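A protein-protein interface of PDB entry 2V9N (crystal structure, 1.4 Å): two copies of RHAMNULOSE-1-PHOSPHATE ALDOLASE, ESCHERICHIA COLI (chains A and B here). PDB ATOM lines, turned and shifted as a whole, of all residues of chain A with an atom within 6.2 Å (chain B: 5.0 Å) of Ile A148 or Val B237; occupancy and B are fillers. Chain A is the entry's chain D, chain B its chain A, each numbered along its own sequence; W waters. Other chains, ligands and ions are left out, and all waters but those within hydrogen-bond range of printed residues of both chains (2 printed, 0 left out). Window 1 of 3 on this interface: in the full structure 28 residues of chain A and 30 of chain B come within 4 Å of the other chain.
The backbone carbonyl oxygen (O) of Gly B168 sits close to the side-chain hydroxyl (OH) of Tyr A152 (3.5 Å).
NZ of Lys B233 sits at hydrogen-bond distance from O of His A143 (2.8 Å).
The side-chain amide oxygen of Asn A146 is in hydrogen-bond range of the side-chain amino group of Lys B240, at 2.8 Å.
The side-chain carboxylate (OE1) of Glu A232 sits at hydrogen-bond distance from the backbone NH (N) of Thr A145 (3.4 Å).
The side-chain carboxylate (OE1) of Glu A232 sits at hydrogen-bond distance from the backbone NH (N) of Asn A146.
O of Ile A148 lies within hydrogen-bond range of OG1 of Thr A151, 2.7 Å away.
OG1 of Thr A151 lies within hydrogen-bond range of N of Phe A211, at 2.9 Å.
Thr A145 touches Lys B233.
CD of Gln B236 touches CG2 of Thr A145, at 3.7 Å.
Thr A145 touches Lys B240 (CG2 to CE, 3.8 Å).
CG1 of Val B237 touches CG2 of Ile A148 (3.9 Å).
Ala A149 touches Lys B240.
CG2 of Val B241 touches O of Ala A149, 3.6 Å away.
OH of Tyr A152 touches N of Ser B169 (3.8 Å).
CE1 of Tyr A152 touches CG1 of Val B237 (3.8 Å).
Tyr A152 touches Val B241 (CD1 to CG2, 3.7 Å).
O of Phe A211 touches C of Ser B169, 3.8 Å away.
Cys A142 touches none of the printed residues of chain B.
Ile A148 touches just one residue of chain B: Val B237.
Printed residues of chain A within 4 Å of Ser B169: Tyr A152 (3.8 Å) and Phe A211 (3.8 Å).
Printed residues of chain A within 4 Å of Lys B233: His A143 (2.8 Å) and Thr A145 (3.4 Å).
Of chain A, only Ile A148 and Tyr A152 come within 4 Å of Val B237.
The nearest printed residue of chain B that does not touch Asn A146 is Val B237 (6.2 Å).
Hydrophobic or aromatic side chains of chain B within 4 Å of the printed part of chain A: Val B237 and Val B241.
Hydrophobic or aromatic side chains of chain A within 4 Å of the printed part of chain B: His A143, Ile A148, Ala A149 and Tyr A152.
Among the printed residues, no Asp or Glu carboxylate lies within 4 Å of a Lys or Arg side-chain nitrogen of the other chain.
Position printed for both chains: 235.
Water W1 bridges ND2 of Asn A146 (3.0 Å) and NZ of Lys B240 (3.0 Å).
Water W2 lies within hydrogen-bond range of OD1 of Asn A146 (3.2 Å) and NZ of Lys B240 (3.4 Å).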
ATOM      1  N   CYS A 142      10.520 -30.655 -22.535  1.00  0.00           N
ATOM      2  CA  CYS A 142      11.576 -31.633 -22.718  1.00  0.00           C
ATOM      3  C   CYS A 142      12.677 -31.047 -23.567  1.00  0.00           C
ATOM      4  O   CYS A 142      12.541 -29.961 -24.135  1.00  0.00           O
ATOM      5  CB  CYS A 142      11.019 -32.916 -23.335  1.00  0.00           C
ATOM      6  SG  CYS A 142      10.441 -32.701 -25.025  1.00  0.00           S
ATOM      7  N   HIS A 143      13.779 -31.783 -23.641  1.00  0.00           N
ATOM      8  CA  HIS A 143      14.961 -31.341 -24.341  1.00  0.00           C
ATOM      9  C   HIS A 143      15.012 -32.009 -25.722  1.00  0.00           C
ATOM     10  O   HIS A 143      15.828 -32.886 -25.986  1.00  0.00           O
ATOM     11  CB  HIS A 143      16.183 -31.614 -23.471  1.00  0.00           C
ATOM     12  CG  HIS A 143      16.192 -30.817 -22.198  1.00  0.00           C
ATOM     13  ND1 HIS A 143      17.132 -31.000 -21.212  1.00  0.00           N
ATOM     14  CD2 HIS A 143      15.393 -29.809 -21.776  1.00  0.00           C
ATOM     15  CE1 HIS A 143      16.913 -30.135 -20.236  1.00  0.00           C
ATOM     16  NE2 HIS A 143      15.859 -29.403 -20.550  1.00  0.00           N
ATOM     17  N   ALA A 144      14.098 -31.584 -26.596  1.00  0.00           N
ATOM     18  CA  ALA A 144      13.901 -32.196 -27.908  1.00  0.00           C
ATOM     19  C   ALA A 144      15.104 -31.880 -28.793  1.00  0.00           C
ATOM     20  O   ALA A 144      15.327 -30.744 -29.181  1.00  0.00           O
ATOM     21  CB  ALA A 144      12.615 -31.700 -28.534  1.00  0.00           C
ATOM     22  N   THR A 145      15.873 -32.920 -29.094  1.00  0.00           N
ATOM     23  CA  THR A 145      17.232 -32.821 -29.626  1.00  0.00           C
ATOM     24  C   THR A 145      17.389 -31.986 -30.888  1.00  0.00           C
ATOM     25  O   THR A 145      18.230 -31.086 -30.952  1.00  0.00           O
ATOM     26  CB  THR A 145      17.778 -34.236 -29.915  1.00  0.00           C
ATOM     27  OG1 THR A 145      17.519 -35.088 -28.803  1.00  0.00           O
ATOM     28  CG2 THR A 145      19.293 -34.224 -30.176  1.00  0.00           C
ATOM     29  N   ASN A 146      16.580 -32.285 -31.898  1.00  0.00           N
ATOM     30  CA  ASN A 146      16.678 -31.571 -33.167  1.00  0.00           C
ATOM     31  C   ASN A 146      16.138 -30.151 -33.097  1.00  0.00           C
ATOM     32  O   ASN A 146      16.707 -29.243 -33.689  1.00  0.00           O
ATOM     33  CB  ASN A 146      15.997 -32.378 -34.263  1.00  0.00           C
ATOM     34  CG  ASN A 146      16.728 -33.658 -34.556  1.00  0.00           C
ATOM     35  OD1 ASN A 146      17.746 -33.654 -35.252  1.00  0.00           O
ATOM     36  ND2 ASN A 146      16.203 -34.774 -34.039  1.00  0.00           N
ATOM     37  N   LEU A 147      15.059 -29.937 -32.356  1.00  0.00           N
ATOM     38  CA  LEU A 147      14.592 -28.570 -32.118  1.00  0.00           C
ATOM     39  C   LEU A 147      15.695 -27.739 -31.439  1.00  0.00           C
ATOM     40  O   LEU A 147      15.928 -26.595 -31.822  1.00  0.00           O
ATOM     41  CB  LEU A 147      13.318 -28.552 -31.274  1.00  0.00           C
ATOM     42  CG  LEU A 147      12.060 -28.959 -32.045  1.00  0.00           C
ATOM     43  CD1 LEU A 147      10.929 -29.336 -31.089  1.00  0.00           C
ATOM     44  CD2 LEU A 147      11.613 -27.839 -33.003  1.00  0.00           C
ATOM     45  N   ILE A 148      16.389 -28.315 -30.463  1.00  0.00           N
ATOM     46  CA  ILE A 148      17.504 -27.618 -29.820  1.00  0.00           C
ATOM     47  C   ILE A 148      18.580 -27.267 -30.861  1.00  0.00           C
ATOM     48  O   ILE A 148      19.038 -26.115 -30.962  1.00  0.00           O
ATOM     49  CB  ILE A 148      18.113 -28.457 -28.666  1.00  0.00           C
ATOM     50  CG1 ILE A 148      17.103 -28.618 -27.523  1.00  0.00           C
ATOM     51  CG2 ILE A 148      19.414 -27.811 -28.125  1.00  0.00           C
ATOM     52  CD1 ILE A 148      17.445 -29.730 -26.563  1.00  0.00           C
ATOM     53  N   ALA A 149      18.971 -28.250 -31.658  1.00  0.00           N
ATOM     54  CA  ALA A 149      20.029 -28.017 -32.641  1.00  0.00           C
ATOM     55  C   ALA A 149      19.669 -26.883 -33.594  1.00  0.00           C
ATOM     56  O   ALA A 149      20.507 -26.039 -33.930  1.00  0.00           O
ATOM     57  CB  ALA A 149      20.352 -29.281 -33.431  1.00  0.00           C
ATOM     58  N   LEU A 150      18.422 -26.858 -34.047  1.00  0.00           N
ATOM     59  CA  LEU A 150      18.007 -25.805 -34.978  1.00  0.00           C
ATOM     60  C   LEU A 150      18.126 -24.398 -34.397  1.00  0.00           C
ATOM     61  O   LEU A 150      18.340 -23.452 -35.140  1.00  0.00           O
ATOM     62  CB  LEU A 150      16.570 -26.015 -35.451  1.00  0.00           C
ATOM     63  CG  LEU A 150      16.344 -27.203 -36.387  1.00  0.00           C
ATOM     64  CD1 LEU A 150      14.859 -27.273 -36.786  1.00  0.00           C
ATOM     65  CD2 LEU A 150      17.236 -27.124 -37.615  1.00  0.00           C
ATOM     66  N   THR A 151      18.002 -24.246 -33.082  1.00  0.00           N
ATOM     67  CA  THR A 151      18.103 -22.916 -32.484  1.00  0.00           C
ATOM     68  C   THR A 151      19.508 -22.313 -32.593  1.00  0.00           C
ATOM     69  O   THR A 151      19.670 -21.114 -32.312  1.00  0.00           O
ATOM     70  CB  THR A 151      17.629 -22.877 -31.008  1.00  0.00           C
ATOM     71  OG1 THR A 151      18.514 -23.635 -30.169  1.00  0.00           O
ATOM     72  CG2 THR A 151      16.207 -23.403 -30.884  1.00  0.00           C
ATOM     73  N   TYR A 152      20.518 -23.104 -32.978  1.00  0.00           N
ATOM     74  CA  TYR A 152      21.872 -22.555 -33.223  1.00  0.00           C
ATOM     75  C   TYR A 152      22.112 -22.165 -34.677  1.00  0.00           C
ATOM     76  O   TYR A 152      23.132 -21.535 -34.991  1.00  0.00           O
ATOM     77  CB  TYR A 152      22.972 -23.556 -32.832  1.00  0.00           C
ATOM     78  CG  TYR A 152      22.938 -24.013 -31.378  1.00  0.00           C
ATOM     79  CD1 TYR A 152      22.037 -24.983 -30.957  1.00  0.00           C
ATOM     80  CD2 TYR A 152      23.813 -23.482 -30.437  1.00  0.00           C
ATOM     81  CE1 TYR A 152      21.995 -25.399 -29.647  1.00  0.00           C
ATOM     82  CE2 TYR A 152      23.776 -23.881 -29.127  1.00  0.00           C
ATOM     83  CZ  TYR A 152      22.870 -24.847 -28.729  1.00  0.00           C
ATOM     84  OH  TYR A 152      22.821 -25.259 -27.424  1.00  0.00           O
ATOM     85  N   LEU A 208       9.587 -22.362 -27.879  1.00  0.00           N
ATOM     86  CA  LEU A 208      10.983 -22.794 -27.829  1.00  0.00           C
ATOM     87  C   LEU A 208      11.830 -21.898 -26.931  1.00  0.00           C
ATOM     88  O   LEU A 208      11.676 -20.673 -26.939  1.00  0.00           O
ATOM     89  CB  LEU A 208      11.602 -22.799 -29.229  1.00  0.00           C
ATOM     90  CG  LEU A 208      11.108 -23.907 -30.164  1.00  0.00           C
ATOM     91  CD1 LEU A 208      11.612 -23.671 -31.571  1.00  0.00           C
ATOM     92  CD2 LEU A 208      11.512 -25.300 -29.653  1.00  0.00           C
ATOM     93  N   TRP A 209      12.732 -22.552 -26.191  1.00  0.00           N
ATOM     94  CA  TRP A 209      13.764 -21.957 -25.361  1.00  0.00           C
ATOM     95  C   TRP A 209      15.075 -22.209 -26.097  1.00  0.00           C
ATOM     96  O   TRP A 209      15.567 -23.343 -26.103  1.00  0.00           O
ATOM     97  CB  TRP A 209      13.787 -22.669 -24.008  1.00  0.00           C
ATOM     98  CG  TRP A 209      12.671 -22.257 -23.081  1.00  0.00           C
ATOM     99  CD1 TRP A 209      11.589 -21.475 -23.383  1.00  0.00           C
ATOM    100  CD2 TRP A 209      12.532 -22.622 -21.703  1.00  0.00           C
ATOM    101  NE1 TRP A 209      10.802 -21.314 -22.265  1.00  0.00           N
ATOM    102  CE2 TRP A 209      11.355 -22.011 -21.224  1.00  0.00           C
ATOM    103  CE3 TRP A 209      13.290 -23.403 -20.826  1.00  0.00           C
ATOM    104  CZ2 TRP A 209      10.928 -22.143 -19.898  1.00  0.00           C
ATOM    105  CZ3 TRP A 209      12.861 -23.542 -19.506  1.00  0.00           C
ATOM    106  CH2 TRP A 209      11.693 -22.901 -19.057  1.00  0.00           C
ATOM    107  N   PRO A 210      15.636 -21.177 -26.744  1.00  0.00           N
ATOM    108  CA  PRO A 210      16.856 -21.421 -27.508  1.00  0.00           C
ATOM    109  C   PRO A 210      17.960 -22.086 -26.685  1.00  0.00           C
ATOM    110  O   PRO A 210      18.104 -21.792 -25.498  1.00  0.00           O
ATOM    111  CB  PRO A 210      17.279 -20.020 -27.956  1.00  0.00           C
ATOM    112  CG  PRO A 210      16.016 -19.234 -27.966  1.00  0.00           C
ATOM    113  CD  PRO A 210      15.202 -19.768 -26.835  1.00  0.00           C
ATOM    114  N   PHE A 211      18.711 -22.990 -27.319  1.00  0.00           N
ATOM    115  CA  PHE A 211      19.858 -23.657 -26.695  1.00  0.00           C
ATOM    116  C   PHE A 211      19.431 -24.486 -25.475  1.00  0.00           C
ATOM    117  O   PHE A 211      20.246 -24.768 -24.583  1.00  0.00           O
ATOM    118  CB  PHE A 211      20.954 -22.642 -26.292  1.00  0.00           C
ATOM    119  CG  PHE A 211      21.116 -21.484 -27.250  1.00  0.00           C
ATOM    120  CD1 PHE A 211      21.167 -20.175 -26.771  1.00  0.00           C
ATOM    121  CD2 PHE A 211      21.199 -21.691 -28.621  1.00  0.00           C
ATOM    122  CE1 PHE A 211      21.313 -19.089 -27.641  1.00  0.00           C
ATOM    123  CE2 PHE A 211      21.345 -20.612 -29.492  1.00  0.00           C
ATOM    124  CZ  PHE A 211      21.402 -19.315 -28.997  1.00  0.00           C
ATOM    125  N   HIS A 212      18.163 -24.900 -25.455  1.00  0.00           N
ATOM    126  CA  HIS A 212      17.597 -25.532 -24.260  1.00  0.00           C
ATOM    127  C   HIS A 212      16.493 -26.550 -24.595  1.00  0.00           C
ATOM    128  O   HIS A 212      16.672 -27.741 -24.376  1.00  0.00           O
ATOM    129  CB  HIS A 212      17.094 -24.462 -23.277  1.00  0.00           C
ATOM    130  CG  HIS A 212      16.589 -25.019 -21.978  1.00  0.00           C
ATOM    131  ND1 HIS A 212      16.531 -24.268 -20.822  1.00  0.00           N
ATOM    132  CD2 HIS A 212      16.155 -26.257 -21.642  1.00  0.00           C
ATOM    133  CE1 HIS A 212      16.050 -25.017 -19.841  1.00  0.00           C
ATOM    134  NE2 HIS A 212      15.809 -26.227 -20.315  1.00  0.00           N
ATOM    135  N   GLY A 213      15.341 -26.115 -25.103  1.00  0.00           N
ATOM    136  CA  GLY A 213      14.289 -27.104 -25.379  1.00  0.00           C
ATOM    137  C   GLY A 213      12.966 -26.489 -25.734  1.00  0.00           C
ATOM    138  O   GLY A 213      12.926 -25.387 -26.270  1.00  0.00           O
ATOM    139  N   VAL A 214      11.896 -27.217 -25.427  1.00  0.00           N
ATOM    140  CA  VAL A 214      10.557 -26.887 -25.894  1.00  0.00           C
ATOM    141  C   VAL A 214       9.551 -27.030 -24.762  1.00  0.00           C
ATOM    142  O   VAL A 214       9.762 -27.822 -23.835  1.00  0.00           O
ATOM    143  CB  VAL A 214      10.158 -27.798 -27.101  1.00  0.00           C
ATOM    144  CG1 VAL A 214      10.041 -29.279 -26.681  1.00  0.00           C
ATOM    145  CG2 VAL A 214       8.865 -27.302 -27.775  1.00  0.00           C
ATOM    146  N   GLU A 232       9.196 -31.990 -33.326  1.00  0.00           N
ATOM    147  CA  GLU A 232      10.543 -32.584 -33.254  1.00  0.00           C
ATOM    148  C   GLU A 232      10.868 -33.479 -34.450  1.00  0.00           C
ATOM    149  O   GLU A 232      12.012 -33.539 -34.894  1.00  0.00           O
ATOM    150  CB  GLU A 232      10.697 -33.362 -31.938  1.00  0.00           C
ATOM    151  CG  GLU A 232      11.989 -34.171 -31.783  1.00  0.00           C
ATOM    152  CD  GLU A 232      13.269 -33.370 -31.864  1.00  0.00           C
ATOM    153  OE1 GLU A 232      14.333 -34.017 -31.969  1.00  0.00           O
ATOM    154  OE2 GLU A 232      13.223 -32.135 -31.784  1.00  0.00           O
ATOM    155  N   ALA A 235      11.710 -31.099 -37.167  1.00  0.00           N
ATOM    156  CA  ALA A 235      13.074 -30.653 -36.886  1.00  0.00           C
ATOM    157  C   ALA A 235      14.108 -31.694 -37.298  1.00  0.00           C
ATOM    158  O   ALA A 235      15.146 -31.342 -37.834  1.00  0.00           O
ATOM    159  CB  ALA A 235      13.255 -30.303 -35.385  1.00  0.00           C
ATOM    160  N   GLY B 168      26.263 -26.303 -25.740  1.00  0.00           N
ATOM    161  CA  GLY B 168      25.408 -27.247 -26.478  1.00  0.00           C
ATOM    162  C   GLY B 168      24.155 -27.724 -25.757  1.00  0.00           C
ATOM    163  O   GLY B 168      23.361 -28.487 -26.326  1.00  0.00           O
ATOM    164  N   SER B 169      23.981 -27.315 -24.501  1.00  0.00           N
ATOM    165  CA  SER B 169      22.708 -27.509 -23.784  1.00  0.00           C
ATOM    166  C   SER B 169      22.777 -26.642 -22.537  1.00  0.00           C
ATOM    167  O   SER B 169      23.757 -26.686 -21.816  1.00  0.00           O
ATOM    168  CB  SER B 169      22.457 -28.971 -23.386  1.00  0.00           C
ATOM    169  OG  SER B 169      22.061 -29.761 -24.495  1.00  0.00           O
ATOM    170  N   LYS B 233      24.624 -35.733 -24.519  1.00  0.00           N
ATOM    171  CA  LYS B 233      23.497 -35.071 -25.156  1.00  0.00           C
ATOM    172  C   LYS B 233      23.938 -33.746 -25.784  1.00  0.00           C
ATOM    173  O   LYS B 233      23.589 -33.406 -26.929  1.00  0.00           O
ATOM    174  CB  LYS B 233      22.369 -34.838 -24.143  1.00  0.00           C
ATOM    175  CG  LYS B 233      21.224 -33.950 -24.635  1.00  0.00           C
ATOM    176  CD  LYS B 233      20.559 -34.481 -25.895  1.00  0.00           C
ATOM    177  CE  LYS B 233      19.208 -33.802 -26.130  1.00  0.00           C
ATOM    178  NZ  LYS B 233      18.114 -34.303 -25.199  1.00  0.00           N
ATOM    179  N   SER B 234      24.689 -32.966 -25.019  1.00  0.00           N
ATOM    180  CA  SER B 234      25.263 -31.741 -25.570  1.00  0.00           C
ATOM    181  C   SER B 234      26.140 -32.029 -26.795  1.00  0.00           C
ATOM    182  O   SER B 234      26.059 -31.359 -27.817  1.00  0.00           O
ATOM    183  CB  SER B 234      26.077 -31.016 -24.494  1.00  0.00           C
ATOM    184  OG  SER B 234      26.614 -29.833 -25.003  1.00  0.00           O
ATOM    185  N   ALA B 235      26.990 -33.042 -26.695  1.00  0.00           N
ATOM    186  CA  ALA B 235      27.806 -33.440 -27.838  1.00  0.00           C
ATOM    187  C   ALA B 235      26.972 -33.824 -29.066  1.00  0.00           C
ATOM    188  O   ALA B 235      27.332 -33.505 -30.181  1.00  0.00           O
ATOM    189  CB  ALA B 235      28.705 -34.602 -27.464  1.00  0.00           C
ATOM    190  N   GLN B 236      25.872 -34.530 -28.842  1.00  0.00           N
ATOM    191  CA  GLN B 236      24.953 -34.912 -29.906  1.00  0.00           C
ATOM    192  C   GLN B 236      24.384 -33.686 -30.610  1.00  0.00           C
ATOM    193  O   GLN B 236      24.292 -33.638 -31.846  1.00  0.00           O
ATOM    194  CB  GLN B 236      23.814 -35.745 -29.311  1.00  0.00           C
ATOM    195  CG  GLN B 236      22.847 -36.267 -30.373  1.00  0.00           C
ATOM    196  CD  GLN B 236      21.662 -37.026 -29.813  1.00  0.00           C
ATOM    197  OE1 GLN B 236      21.406 -37.031 -28.604  1.00  0.00           O
ATOM    198  NE2 GLN B 236      20.917 -37.671 -30.706  1.00  0.00           N
ATOM    199  N   VAL B 237      23.979 -32.701 -29.817  1.00  0.00           N
ATOM    200  CA  VAL B 237      23.491 -31.437 -30.363  1.00  0.00           C
ATOM    201  C   VAL B 237      24.591 -30.754 -31.180  1.00  0.00           C
ATOM    202  O   VAL B 237      24.372 -30.320 -32.314  1.00  0.00           O
ATOM    203  CB  VAL B 237      22.993 -30.507 -29.252  1.00  0.00           C
ATOM    204  CG1 VAL B 237      22.744 -29.112 -29.801  1.00  0.00           C
ATOM    205  CG2 VAL B 237      21.703 -31.064 -28.624  1.00  0.00           C
ATOM    206  N   LEU B 238      25.785 -30.679 -30.612  1.00  0.00           N
ATOM    207  CA  LEU B 238      26.905 -30.033 -31.306  1.00  0.00           C
ATOM    208  C   LEU B 238      27.228 -30.714 -32.638  1.00  0.00           C
ATOM    209  O   LEU B 238      27.515 -30.055 -33.621  1.00  0.00           O
ATOM    210  CB  LEU B 238      28.157 -30.005 -30.428  1.00  0.00           C
ATOM    211  CG  LEU B 238      28.086 -29.123 -29.189  1.00  0.00           C
ATOM    212  CD1 LEU B 238      29.335 -29.317 -28.337  1.00  0.00           C
ATOM    213  CD2 LEU B 238      27.902 -27.635 -29.541  1.00  0.00           C
ATOM    214  N   VAL B 239      27.208 -32.039 -32.664  1.00  0.00           N
ATOM    215  CA  VAL B 239      27.501 -32.749 -33.912  1.00  0.00           C
ATOM    216  C   VAL B 239      26.482 -32.360 -34.984  1.00  0.00           C
ATOM    217  O   VAL B 239      26.846 -32.151 -36.144  1.00  0.00           O
ATOM    218  CB  VAL B 239      27.587 -34.274 -33.695  1.00  0.00           C
ATOM    219  CG1 VAL B 239      27.595 -35.048 -35.048  1.00  0.00           C
ATOM    220  CG2 VAL B 239      28.813 -34.592 -32.830  1.00  0.00           C
ATOM    221  N   LYS B 240      25.205 -32.248 -34.615  1.00  0.00           N
ATOM    222  CA  LYS B 240      24.199 -31.792 -35.580  1.00  0.00           C
ATOM    223  C   LYS B 240      24.517 -30.373 -36.054  1.00  0.00           C
ATOM    224  O   LYS B 240      24.482 -30.088 -37.243  1.00  0.00           O
ATOM    225  CB  LYS B 240      22.797 -31.840 -34.966  1.00  0.00           C
ATOM    226  CG  LYS B 240      22.301 -33.260 -34.737  1.00  0.00           C
ATOM    227  CD  LYS B 240      20.975 -33.274 -34.011  1.00  0.00           C
ATOM    228  CE  LYS B 240      20.489 -34.697 -33.743  1.00  0.00           C
ATOM    229  NZ  LYS B 240      19.956 -35.355 -34.970  1.00  0.00           N
ATOM    230  N   VAL B 241      24.810 -29.490 -35.108  1.00  0.00           N
ATOM    231  CA  VAL B 241      25.038 -28.082 -35.424  1.00  0.00           C
ATOM    232  C   VAL B 241      26.242 -27.930 -36.339  1.00  0.00           C
ATOM    233  O   VAL B 241      26.179 -27.221 -37.342  1.00  0.00           O
ATOM    234  CB  VAL B 241      25.224 -27.222 -34.154  1.00  0.00           C
ATOM    235  CG1 VAL B 241      25.717 -25.821 -34.522  1.00  0.00           C
ATOM    236  CG2 VAL B 241      23.924 -27.154 -33.351  1.00  0.00           C
HETATM  237  O   HOH W   1      17.785 -37.273 -34.202  1.00  0.00           O
HETATM  238  O   HOH W   2      18.297 -35.384 -37.927  1.00  0.00           O
